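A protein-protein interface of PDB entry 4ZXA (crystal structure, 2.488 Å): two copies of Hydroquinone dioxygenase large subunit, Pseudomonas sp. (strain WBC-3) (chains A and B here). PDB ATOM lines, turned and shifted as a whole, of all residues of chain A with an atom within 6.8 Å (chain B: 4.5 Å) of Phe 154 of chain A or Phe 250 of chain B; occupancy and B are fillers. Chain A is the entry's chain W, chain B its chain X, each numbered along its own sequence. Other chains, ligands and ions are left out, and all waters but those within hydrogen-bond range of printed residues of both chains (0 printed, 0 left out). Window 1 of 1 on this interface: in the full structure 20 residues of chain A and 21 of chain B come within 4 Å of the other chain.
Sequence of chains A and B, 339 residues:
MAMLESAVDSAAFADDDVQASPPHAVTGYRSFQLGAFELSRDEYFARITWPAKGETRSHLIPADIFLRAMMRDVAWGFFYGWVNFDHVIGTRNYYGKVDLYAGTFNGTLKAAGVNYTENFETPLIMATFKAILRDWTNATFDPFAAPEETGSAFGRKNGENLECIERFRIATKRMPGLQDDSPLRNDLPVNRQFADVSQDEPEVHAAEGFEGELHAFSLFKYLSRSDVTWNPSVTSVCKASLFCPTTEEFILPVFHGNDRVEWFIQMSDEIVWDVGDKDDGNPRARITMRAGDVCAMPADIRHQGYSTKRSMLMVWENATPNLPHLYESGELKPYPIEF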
ATOM      1  N   TYR A  29       1.750  -7.994  24.717  1.00  0.00           N
ATOM      2  CA  TYR A  29       2.610  -8.915  25.449  1.00  0.00           C
ATOM      3  C   TYR A  29       1.863  -9.606  26.583  1.00  0.00           C
ATOM      4  O   TYR A  29       0.902  -9.074  27.118  1.00  0.00           O
ATOM      5  CB  TYR A  29       3.832  -8.191  26.034  1.00  0.00           C
ATOM      6  CG  TYR A  29       4.711  -7.452  25.038  1.00  0.00           C
ATOM      7  CD1 TYR A  29       5.460  -8.141  24.090  1.00  0.00           C
ATOM      8  CD2 TYR A  29       4.825  -6.065  25.073  1.00  0.00           C
ATOM      9  CE1 TYR A  29       6.276  -7.469  23.190  1.00  0.00           C
ATOM     10  CE2 TYR A  29       5.639  -5.388  24.176  1.00  0.00           C
ATOM     11  CZ  TYR A  29       6.359  -6.099  23.241  1.00  0.00           C
ATOM     12  OH  TYR A  29       7.159  -5.430  22.343  1.00  0.00           O
ATOM     13  N   ARG A  41       5.981  -6.618  30.555  1.00  0.00           N
ATOM     14  CA  ARG A  41       6.724  -5.627  29.795  1.00  0.00           C
ATOM     15  C   ARG A  41       5.782  -4.737  29.001  1.00  0.00           C
ATOM     16  O   ARG A  41       4.696  -5.154  28.618  1.00  0.00           O
ATOM     17  CB  ARG A  41       7.726  -6.304  28.858  1.00  0.00           C
ATOM     18  CG  ARG A  41       7.149  -6.716  27.521  1.00  0.00           C
ATOM     19  CD  ARG A  41       8.196  -6.673  26.427  1.00  0.00           C
ATOM     20  NE  ARG A  41       8.435  -5.317  25.949  1.00  0.00           N
ATOM     21  CZ  ARG A  41       9.247  -5.008  24.945  1.00  0.00           C
ATOM     22  NH1 ARG A  41       9.905  -5.958  24.304  1.00  0.00           N
ATOM     23  NH2 ARG A  41       9.401  -3.746  24.581  1.00  0.00           N
ATOM     24  N   ASP A  42       6.206  -3.504  28.761  1.00  0.00           N
ATOM     25  CA  ASP A  42       5.459  -2.602  27.905  1.00  0.00           C
ATOM     26  C   ASP A  42       6.321  -2.189  26.721  1.00  0.00           C
ATOM     27  O   ASP A  42       7.188  -2.938  26.290  1.00  0.00           O
ATOM     28  CB  ASP A  42       4.964  -1.378  28.679  1.00  0.00           C
ATOM     29  CG  ASP A  42       6.079  -0.629  29.359  1.00  0.00           C
ATOM     30  OD1 ASP A  42       7.234  -0.763  28.923  1.00  0.00           O
ATOM     31  OD2 ASP A  42       5.799   0.096  30.329  1.00  0.00           O
ATOM     32  N   GLU A  43       6.078  -0.999  26.195  1.00  0.00           N
ATOM     33  CA  GLU A  43       6.779  -0.539  25.007  1.00  0.00           C
ATOM     34  C   GLU A  43       8.250  -0.217  25.269  1.00  0.00           C
ATOM     35  O   GLU A  43       9.066  -0.239  24.354  1.00  0.00           O
ATOM     36  CB  GLU A  43       6.063   0.669  24.403  1.00  0.00           C
ATOM     37  CG  GLU A  43       4.699   0.350  23.812  1.00  0.00           C
ATOM     38  CD  GLU A  43       3.577   0.445  24.827  1.00  0.00           C
ATOM     39  OE1 GLU A  43       3.866   0.583  26.028  1.00  0.00           O
ATOM     40  OE2 GLU A  43       2.402   0.381  24.422  1.00  0.00           O
ATOM     41  N   TYR A  44       8.584   0.081  26.518  1.00  0.00           N
ATOM     42  CA  TYR A  44       9.957   0.442  26.869  1.00  0.00           C
ATOM     43  C   TYR A  44      10.595  -0.402  27.982  1.00  0.00           C
ATOM     44  O   TYR A  44      11.813  -0.577  28.001  1.00  0.00           O
ATOM     45  CB  TYR A  44      10.029   1.914  27.289  1.00  0.00           C
ATOM     46  CG  TYR A  44      10.145   2.907  26.153  1.00  0.00           C
ATOM     47  CD1 TYR A  44       9.162   3.867  25.941  1.00  0.00           C
ATOM     48  CD2 TYR A  44      11.234   2.891  25.302  1.00  0.00           C
ATOM     49  CE1 TYR A  44       9.271   4.781  24.921  1.00  0.00           C
ATOM     50  CE2 TYR A  44      11.351   3.803  24.275  1.00  0.00           C
ATOM     51  CZ  TYR A  44      10.366   4.748  24.085  1.00  0.00           C
ATOM     52  OH  TYR A  44      10.478   5.660  23.052  1.00  0.00           O
ATOM     53  N   PHE A  45       9.794  -0.906  28.920  1.00  0.00           N
ATOM     54  CA  PHE A  45      10.362  -1.532  30.110  1.00  0.00           C
ATOM     55  C   PHE A  45       9.853  -2.930  30.427  1.00  0.00           C
ATOM     56  O   PHE A  45       8.667  -3.231  30.293  1.00  0.00           O
ATOM     57  CB  PHE A  45      10.142  -0.654  31.340  1.00  0.00           C
ATOM     58  CG  PHE A  45      10.402   0.805  31.103  1.00  0.00           C
ATOM     59  CD1 PHE A  45      11.697   1.278  30.948  1.00  0.00           C
ATOM     60  CD2 PHE A  45       9.351   1.711  31.047  1.00  0.00           C
ATOM     61  CE1 PHE A  45      11.949   2.624  30.724  1.00  0.00           C
ATOM     62  CE2 PHE A  45       9.593   3.065  30.831  1.00  0.00           C
ATOM     63  CZ  PHE A  45      10.893   3.523  30.666  1.00  0.00           C
ATOM     64  N   PRO A  62      14.851  -1.266  31.283  1.00  0.00           N
ATOM     65  CA  PRO A  62      14.705  -1.077  29.828  1.00  0.00           C
ATOM     66  C   PRO A  62      14.708  -2.434  29.116  1.00  0.00           C
ATOM     67  O   PRO A  62      15.554  -3.274  29.425  1.00  0.00           O
ATOM     68  CB  PRO A  62      15.963  -0.298  29.445  1.00  0.00           C
ATOM     69  CG  PRO A  62      16.344   0.433  30.715  1.00  0.00           C
ATOM     70  CD  PRO A  62      15.978  -0.500  31.842  1.00  0.00           C
ATOM     71  N   ALA A  63      13.786  -2.625  28.174  1.00  0.00           N
ATOM     72  CA  ALA A  63      13.495  -3.936  27.605  1.00  0.00           C
ATOM     73  C   ALA A  63      14.680  -4.572  26.903  1.00  0.00           C
ATOM     74  O   ALA A  63      14.845  -5.796  26.945  1.00  0.00           O
ATOM     75  CB  ALA A  63      12.301  -3.848  26.650  1.00  0.00           C
ATOM     76  N   ASP A  64      15.496  -3.762  26.236  1.00  0.00           N
ATOM     77  CA  ASP A  64      16.671  -4.334  25.593  1.00  0.00           C
ATOM     78  C   ASP A  64      17.673  -4.843  26.635  1.00  0.00           C
ATOM     79  O   ASP A  64      18.146  -5.966  26.533  1.00  0.00           O
ATOM     80  CB  ASP A  64      17.320  -3.383  24.578  1.00  0.00           C
ATOM     81  CG  ASP A  64      17.725  -2.049  25.184  1.00  0.00           C
ATOM     82  OD1 ASP A  64      17.291  -1.736  26.317  1.00  0.00           O
ATOM     83  OD2 ASP A  64      18.476  -1.302  24.503  1.00  0.00           O
ATOM     84  N   ILE A  65      17.965  -4.036  27.650  1.00  0.00           N
ATOM     85  CA  ILE A  65      18.849  -4.458  28.736  1.00  0.00           C
ATOM     86  C   ILE A  65      18.341  -5.752  29.376  1.00  0.00           C
ATOM     87  O   ILE A  65      19.105  -6.718  29.546  1.00  0.00           O
ATOM     88  CB  ILE A  65      19.042  -3.321  29.774  1.00  0.00           C
ATOM     89  CG1 ILE A  65      19.762  -2.146  29.102  1.00  0.00           C
ATOM     90  CG2 ILE A  65      19.811  -3.788  30.985  1.00  0.00           C
ATOM     91  CD1 ILE A  65      20.000  -0.977  30.013  1.00  0.00           C
ATOM     92  N   ASN A 138      10.755  -9.378  19.800  1.00  0.00           N
ATOM     93  CA  ASN A 138      10.153  -9.132  18.510  1.00  0.00           C
ATOM     94  C   ASN A 138      11.101  -9.524  17.409  1.00  0.00           C
ATOM     95  O   ASN A 138      12.284  -9.725  17.658  1.00  0.00           O
ATOM     96  CB  ASN A 138       9.808  -7.653  18.389  1.00  0.00           C
ATOM     97  CG  ASN A 138       8.872  -7.198  19.478  1.00  0.00           C
ATOM     98  OD1 ASN A 138       7.933  -7.915  19.836  1.00  0.00           O
ATOM     99  ND2 ASN A 138       9.136  -6.019  20.037  1.00  0.00           N
ATOM    100  N   THR A 140      12.507  -8.057  15.313  1.00  0.00           N
ATOM    101  CA  THR A 140      13.363  -6.974  14.916  1.00  0.00           C
ATOM    102  C   THR A 140      14.572  -6.866  15.872  1.00  0.00           C
ATOM    103  O   THR A 140      15.457  -6.038  15.685  1.00  0.00           O
ATOM    104  CB  THR A 140      12.511  -5.687  14.902  1.00  0.00           C
ATOM    105  OG1 THR A 140      12.982  -4.770  13.907  1.00  0.00           O
ATOM    106  CG2 THR A 140      12.491  -5.042  16.264  1.00  0.00           C
ATOM    107  N   PHE A 141      14.614  -7.737  16.873  1.00  0.00           N
ATOM    108  CA  PHE A 141      15.602  -7.645  17.947  1.00  0.00           C
ATOM    109  C   PHE A 141      16.239  -8.997  18.294  1.00  0.00           C
ATOM    110  O   PHE A 141      15.552  -9.961  18.620  1.00  0.00           O
ATOM    111  CB  PHE A 141      14.948  -7.035  19.199  1.00  0.00           C
ATOM    112  CG  PHE A 141      15.885  -6.852  20.366  1.00  0.00           C
ATOM    113  CD1 PHE A 141      16.810  -5.812  20.374  1.00  0.00           C
ATOM    114  CD2 PHE A 141      15.818  -7.692  21.474  1.00  0.00           C
ATOM    115  CE1 PHE A 141      17.676  -5.623  21.451  1.00  0.00           C
ATOM    116  CE2 PHE A 141      16.676  -7.509  22.551  1.00  0.00           C
ATOM    117  CZ  PHE A 141      17.613  -6.468  22.536  1.00  0.00           C
ATOM    118  N   GLY A 151      18.256  -4.533  15.583  1.00  0.00           N
ATOM    119  CA  GLY A 151      17.272  -3.464  15.683  1.00  0.00           C
ATOM    120  C   GLY A 151      16.845  -3.160  17.118  1.00  0.00           C
ATOM    121  O   GLY A 151      17.613  -3.331  18.076  1.00  0.00           O
ATOM    122  N   SER A 152      15.601  -2.715  17.266  1.00  0.00           N
ATOM    123  CA  SER A 152      15.086  -2.258  18.547  1.00  0.00           C
ATOM    124  C   SER A 152      14.291  -3.336  19.283  1.00  0.00           C
ATOM    125  O   SER A 152      13.579  -4.125  18.661  1.00  0.00           O
ATOM    126  CB  SER A 152      14.197  -1.029  18.330  1.00  0.00           C
ATOM    127  OG  SER A 152      13.683  -0.526  19.557  1.00  0.00           O
ATOM    128  N   ALA A 153      14.397  -3.359  20.613  1.00  0.00           N
ATOM    129  CA  ALA A 153      13.519  -4.214  21.408  1.00  0.00           C
ATOM    130  C   ALA A 153      12.269  -3.449  21.822  1.00  0.00           C
ATOM    131  O   ALA A 153      11.406  -3.991  22.524  1.00  0.00           O
ATOM    132  CB  ALA A 153      14.239  -4.733  22.635  1.00  0.00           C
ATOM    133  N   PHE A 154      12.185  -2.188  21.396  1.00  0.00           N
ATOM    134  CA  PHE A 154      11.133  -1.300  21.877  1.00  0.00           C
ATOM    135  C   PHE A 154       9.856  -1.366  21.032  1.00  0.00           C
ATOM    136  O   PHE A 154       9.890  -1.691  19.843  1.00  0.00           O
ATOM    137  CB  PHE A 154      11.641   0.139  21.963  1.00  0.00           C
ATOM    138  CG  PHE A 154      12.714   0.342  22.994  1.00  0.00           C
ATOM    139  CD1 PHE A 154      12.650  -0.296  24.227  1.00  0.00           C
ATOM    140  CD2 PHE A 154      13.790   1.176  22.731  1.00  0.00           C
ATOM    141  CE1 PHE A 154      13.646  -0.094  25.189  1.00  0.00           C
ATOM    142  CE2 PHE A 154      14.790   1.373  23.679  1.00  0.00           C
ATOM    143  CZ  PHE A 154      14.714   0.742  24.915  1.00  0.00           C
ATOM    144  N   GLY A 155       8.729  -1.075  21.673  1.00  0.00           N
ATOM    145  CA  GLY A 155       7.459  -0.947  20.983  1.00  0.00           C
ATOM    146  C   GLY A 155       6.496  -2.047  21.380  1.00  0.00           C
ATOM    147  O   GLY A 155       6.695  -2.736  22.382  1.00  0.00           O
ATOM    148  N   ARG A 156       5.453  -2.227  20.586  1.00  0.00           N
ATOM    149  CA  ARG A 156       4.469  -3.244  20.884  1.00  0.00           C
ATOM    150  C   ARG A 156       4.864  -4.595  20.282  1.00  0.00           C
ATOM    151  O   ARG A 156       5.736  -4.672  19.407  1.00  0.00           O
ATOM    152  CB  ARG A 156       3.089  -2.764  20.429  1.00  0.00           C
ATOM    153  CG  ARG A 156       2.695  -1.496  21.158  1.00  0.00           C
ATOM    154  CD  ARG A 156       1.354  -0.937  20.725  1.00  0.00           C
ATOM    155  NE  ARG A 156       0.976   0.212  21.546  1.00  0.00           N
ATOM    156  CZ  ARG A 156       0.020   1.078  21.223  1.00  0.00           C
ATOM    157  NH1 ARG A 156      -0.657   0.925  20.088  1.00  0.00           N
ATOM    158  NH2 ARG A 156      -0.253   2.095  22.030  1.00  0.00           N
ATOM    159  N   ASN A 158       5.567  -7.676  18.189  1.00  0.00           N
ATOM    160  CA  ASN A 158       5.714  -7.587  16.751  1.00  0.00           C
ATOM    161  C   ASN A 158       6.525  -8.731  16.147  1.00  0.00           C
ATOM    162  O   ASN A 158       7.688  -8.560  15.747  1.00  0.00           O
ATOM    163  CB  ASN A 158       6.313  -6.239  16.371  1.00  0.00           C
ATOM    164  CG  ASN A 158       6.299  -6.012  14.879  1.00  0.00           C
ATOM    165  OD1 ASN A 158       6.302  -6.969  14.104  1.00  0.00           O
ATOM    166  ND2 ASN A 158       6.257  -4.748  14.462  1.00  0.00           N
ATOM    167  N   PRO B 147      14.218   7.233  22.227  1.00  0.00           N
ATOM    168  CA  PRO B 147      15.003   6.266  21.447  1.00  0.00           C
ATOM    169  C   PRO B 147      14.265   5.799  20.199  1.00  0.00           C
ATOM    170  O   PRO B 147      14.910   5.471  19.204  1.00  0.00           O
ATOM    171  CB  PRO B 147      15.198   5.096  22.417  1.00  0.00           C
ATOM    172  CG  PRO B 147      14.966   5.682  23.782  1.00  0.00           C
ATOM    173  CD  PRO B 147      13.939   6.762  23.593  1.00  0.00           C
ATOM    174  N   GLU B 148      12.934   5.770  20.262  1.00  0.00           N
ATOM    175  CA  GLU B 148      12.109   5.407  19.113  1.00  0.00           C
ATOM    176  C   GLU B 148      12.026   6.509  18.050  1.00  0.00           C
ATOM    177  O   GLU B 148      11.550   6.267  16.943  1.00  0.00           O
ATOM    178  CB  GLU B 148      10.690   5.038  19.555  1.00  0.00           C
ATOM    179  CG  GLU B 148      10.554   3.673  20.203  1.00  0.00           C
ATOM    180  CD  GLU B 148       9.101   3.360  20.589  1.00  0.00           C
ATOM    181  OE1 GLU B 148       8.847   3.056  21.776  1.00  0.00           O
ATOM    182  OE2 GLU B 148       8.207   3.418  19.713  1.00  0.00           O
ATOM    183  N   TRP B 230      11.790  15.637  28.077  1.00  0.00           N
ATOM    184  CA  TRP B 230      12.428  15.994  29.334  1.00  0.00           C
ATOM    185  C   TRP B 230      13.143  17.328  29.201  1.00  0.00           C
ATOM    186  O   TRP B 230      14.360  17.409  29.276  1.00  0.00           O
ATOM    187  CB  TRP B 230      13.415  14.913  29.784  1.00  0.00           C
ATOM    188  CG  TRP B 230      12.845  13.508  29.841  1.00  0.00           C
ATOM    189  CD1 TRP B 230      12.974  12.530  28.893  1.00  0.00           C
ATOM    190  CD2 TRP B 230      12.080  12.925  30.913  1.00  0.00           C
ATOM    191  NE1 TRP B 230      12.341  11.381  29.310  1.00  0.00           N
ATOM    192  CE2 TRP B 230      11.781  11.602  30.541  1.00  0.00           C
ATOM    193  CE3 TRP B 230      11.619  13.401  32.147  1.00  0.00           C
ATOM    194  CZ2 TRP B 230      11.040  10.750  31.356  1.00  0.00           C
ATOM    195  CZ3 TRP B 230      10.879  12.553  32.952  1.00  0.00           C
ATOM    196  CH2 TRP B 230      10.605  11.244  32.555  1.00  0.00           C
ATOM    197  N   GLU B 249       9.271  11.023  27.763  1.00  0.00           N
ATOM    198  CA  GLU B 249       9.247   9.705  27.154  1.00  0.00           C
ATOM    199  C   GLU B 249      10.485   8.952  27.606  1.00  0.00           C
ATOM    200  O   GLU B 249      11.522   9.557  27.855  1.00  0.00           O
ATOM    201  CB  GLU B 249       9.197   9.804  25.632  1.00  0.00           C
ATOM    202  CG  GLU B 249       8.635   8.576  24.953  1.00  0.00           C
ATOM    203  CD  GLU B 249       8.491   8.754  23.460  1.00  0.00           C
ATOM    204  OE1 GLU B 249       8.221   9.885  23.017  1.00  0.00           O
ATOM    205  OE2 GLU B 249       8.648   7.762  22.728  1.00  0.00           O
ATOM    206  N   PHE B 250      10.376   7.636  27.709  1.00  0.00           N
ATOM    207  CA  PHE B 250      11.491   6.823  28.169  1.00  0.00           C
ATOM    208  C   PHE B 250      11.951   7.239  29.563  1.00  0.00           C
ATOM    209  O   PHE B 250      11.154   7.327  30.487  1.00  0.00           O
ATOM    210  CB  PHE B 250      12.656   6.864  27.181  1.00  0.00           C
ATOM    211  CG  PHE B 250      13.620   5.732  27.347  1.00  0.00           C
ATOM    212  CD1 PHE B 250      13.160   4.445  27.533  1.00  0.00           C
ATOM    213  CD2 PHE B 250      14.983   5.951  27.329  1.00  0.00           C
ATOM    214  CE1 PHE B 250      14.037   3.402  27.694  1.00  0.00           C
ATOM    215  CE2 PHE B 250      15.861   4.910  27.487  1.00  0.00           C
ATOM    216  CZ  PHE B 250      15.388   3.635  27.671  1.00  0.00           C
ATOM    217  N   ILE B 251      13.247   7.471  29.709  1.00  0.00           N
ATOM    218  CA  ILE B 251      13.820   7.827  30.996  1.00  0.00           C
ATOM    219  C   ILE B 251      14.465   9.206  31.006  1.00  0.00           C
ATOM    220  O   ILE B 251      15.230   9.539  30.112  1.00  0.00           O
ATOM    221  CB  ILE B 251      14.891   6.800  31.421  1.00  0.00           C
ATOM    222  CG1 ILE B 251      14.419   5.380  31.123  1.00  0.00           C
ATOM    223  CG2 ILE B 251      15.233   6.957  32.889  1.00  0.00           C
ATOM    224  CD1 ILE B 251      15.423   4.322  31.470  1.00  0.00           C
ATOM    225  N   LEU B 252      14.155  10.003  32.022  1.00  0.00           N
ATOM    226  CA  LEU B 252      14.837  11.274  32.221  1.00  0.00           C
ATOM    227  C   LEU B 252      16.342  11.011  32.132  1.00  0.00           C
ATOM    228  O   LEU B 252      16.882  10.246  32.928  1.00  0.00           O
ATOM    229  CB  LEU B 252      14.490  11.836  33.596  1.00  0.00           C
ATOM    230  CG  LEU B 252      15.270  13.089  33.992  1.00  0.00           C
ATOM    231  CD1 LEU B 252      14.863  14.273  33.134  1.00  0.00           C
ATOM    232  CD2 LEU B 252      15.053  13.384  35.461  1.00  0.00           C
ATOM    233  N   GLY B 305      12.850   9.909  36.449  1.00  0.00           N
ATOM    234  CA  GLY B 305      11.541   9.424  36.045  1.00  0.00           C
ATOM    235  C   GLY B 305      11.506   8.440  34.880  1.00  0.00           C
ATOM    236  O   GLY B 305      12.430   8.351  34.057  1.00  0.00           O
ATOM    237  N   TYR B 306      10.408   7.698  34.807  1.00  0.00           N
ATOM    238  CA  TYR B 306      10.183   6.736  33.748  1.00  0.00           C
ATOM    239  C   TYR B 306       8.786   6.980  33.217  1.00  0.00           C
ATOM    240  O   TYR B 306       7.817   7.064  33.985  1.00  0.00           O
ATOM    241  CB  TYR B 306      10.281   5.316  34.300  1.00  0.00           C
ATOM    242  CG  TYR B 306      11.646   4.951  34.852  1.00  0.00           C
ATOM    243  CD1 TYR B 306      12.148   5.571  35.990  1.00  0.00           C
ATOM    244  CD2 TYR B 306      12.427   3.983  34.231  1.00  0.00           C
ATOM    245  CE1 TYR B 306      13.385   5.245  36.484  1.00  0.00           C
ATOM    246  CE2 TYR B 306      13.666   3.647  34.720  1.00  0.00           C
ATOM    247  CZ  TYR B 306      14.141   4.278  35.847  1.00  0.00           C
ATOM    248  OH  TYR B 306      15.376   3.935  36.338  1.00  0.00           O
ATOM    249  N   SER B 307       8.683   7.120  31.902  1.00  0.00           N
ATOM    250  CA  SER B 307       7.402   7.393  31.287  1.00  0.00           C
ATOM    251  C   SER B 307       7.286   6.546  30.037  1.00  0.00           C
ATOM    252  O   SER B 307       7.943   6.829  29.042  1.00  0.00           O
ATOM    253  CB  SER B 307       7.292   8.873  30.941  1.00  0.00           C
ATOM    254  OG  SER B 307       6.034   9.153  30.365  1.00  0.00           O
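No position is printed for both chains.
Of the 9 pairs that touch across the chains among the printed residues, none has its exchanged pair printed and touching as well.
Hydrophobic or aromatic side chains of chain B within 4 Å of the printed part of chain A: Pro 147, Phe 250, Ile 251 and Tyr 306.
Of the 20 printed residues of chain A, 3 touch a printed residue of chain B.
Hydrophobic or aromatic side chains of chain A that line the printed part of chain B: Tyr 44, Phe 45 and Phe 154.
Among the printed residues, 9 pairs touch across the chains.
Among the printed residues, no Asp or Glu carboxylate lies within 4 Å of a Lys or Arg side-chain nitrogen of the other chain.
The side-chain carboxylate of Glu 148 of chain B sits close to the side-chain hydroxyl of Tyr 44 of chain A (3.3 Å).
OE2 of Glu 249 of chain B lies within hydrogen-bond range of OH of Tyr 44 of chain A (2.8 Å).
Among the printed residues, merely in contact across the chains: Tyr 44 of chain A with Pro 147 of chain B (3.7 Å), Tyr 44 of chain A with Phe 250 of chain B (3.3 Å), Phe 45 of chain A with Phe 250 of chain B (3.8 Å), Phe 45 of chain A with Ile 251 of chain B (3.7 Å), Phe 45 of chain A with Tyr 306 of chain B (3.8 Å), Phe 154 of chain A with Pro 147 of chain B (3.95 Å) and Phe 154 of chain A with Phe 250 of chain B (3.9 Å).
The backbone NH of Tyr 44 of chain A is in hydrogen-bond range of the side-chain carboxylate of Asp 42 of chain A (2.9 Å).
The side-chain carboxylate (OD1) of Asp 42 of chain A sits at hydrogen-bond distance from the backbone NH (N) of Phe 45 of chain A, at 2.6 Å.
The backbone carbonyl oxygen of Tyr 44 of chain A lies within hydrogen-bond range of the backbone NH of Ala 63 of chain A, 2.8 Å away.
The side-chain hydroxyl (OG) of Ser 152 of chain A is in hydrogen-bond range of the backbone NH (N) of Phe 154 of chain A (2.9 Å).
The indole nitrogen (NE1) of Trp 230 of chain B is in hydrogen-bond range of the backbone carbonyl oxygen (O) of Glu 249 of chain B (2.5 Å).
The backbone carbonyl oxygen (O) of Phe 250 of chain B lies within hydrogen-bond range of the backbone NH (N) of Ser 307 of chain B, 2.9 Å away.
Phe 154 of chain A touches two residues of chain B.
Of chain A, only Tyr 44, Phe 45 and Phe 154 come within 4 Å of Phe 250 of chain B.
Of the printed residues of chain A, Glu 148 of chain B touches Tyr 44 (3.2 Å).
Printed residues of chain B within 4 Å of Tyr 44 of chain A: Pro 147 (3.7 Å), Glu 148 (3.2 Å), Glu 249 (2.8 Å) and Phe 250 (3.3 Å).
Ser 152 of chain A touches none of the printed residues of chain B.
The nearest printed residue of chain A that does not touch Pro 147 of chain B is Ser 152 of chain A (6.1 Å).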
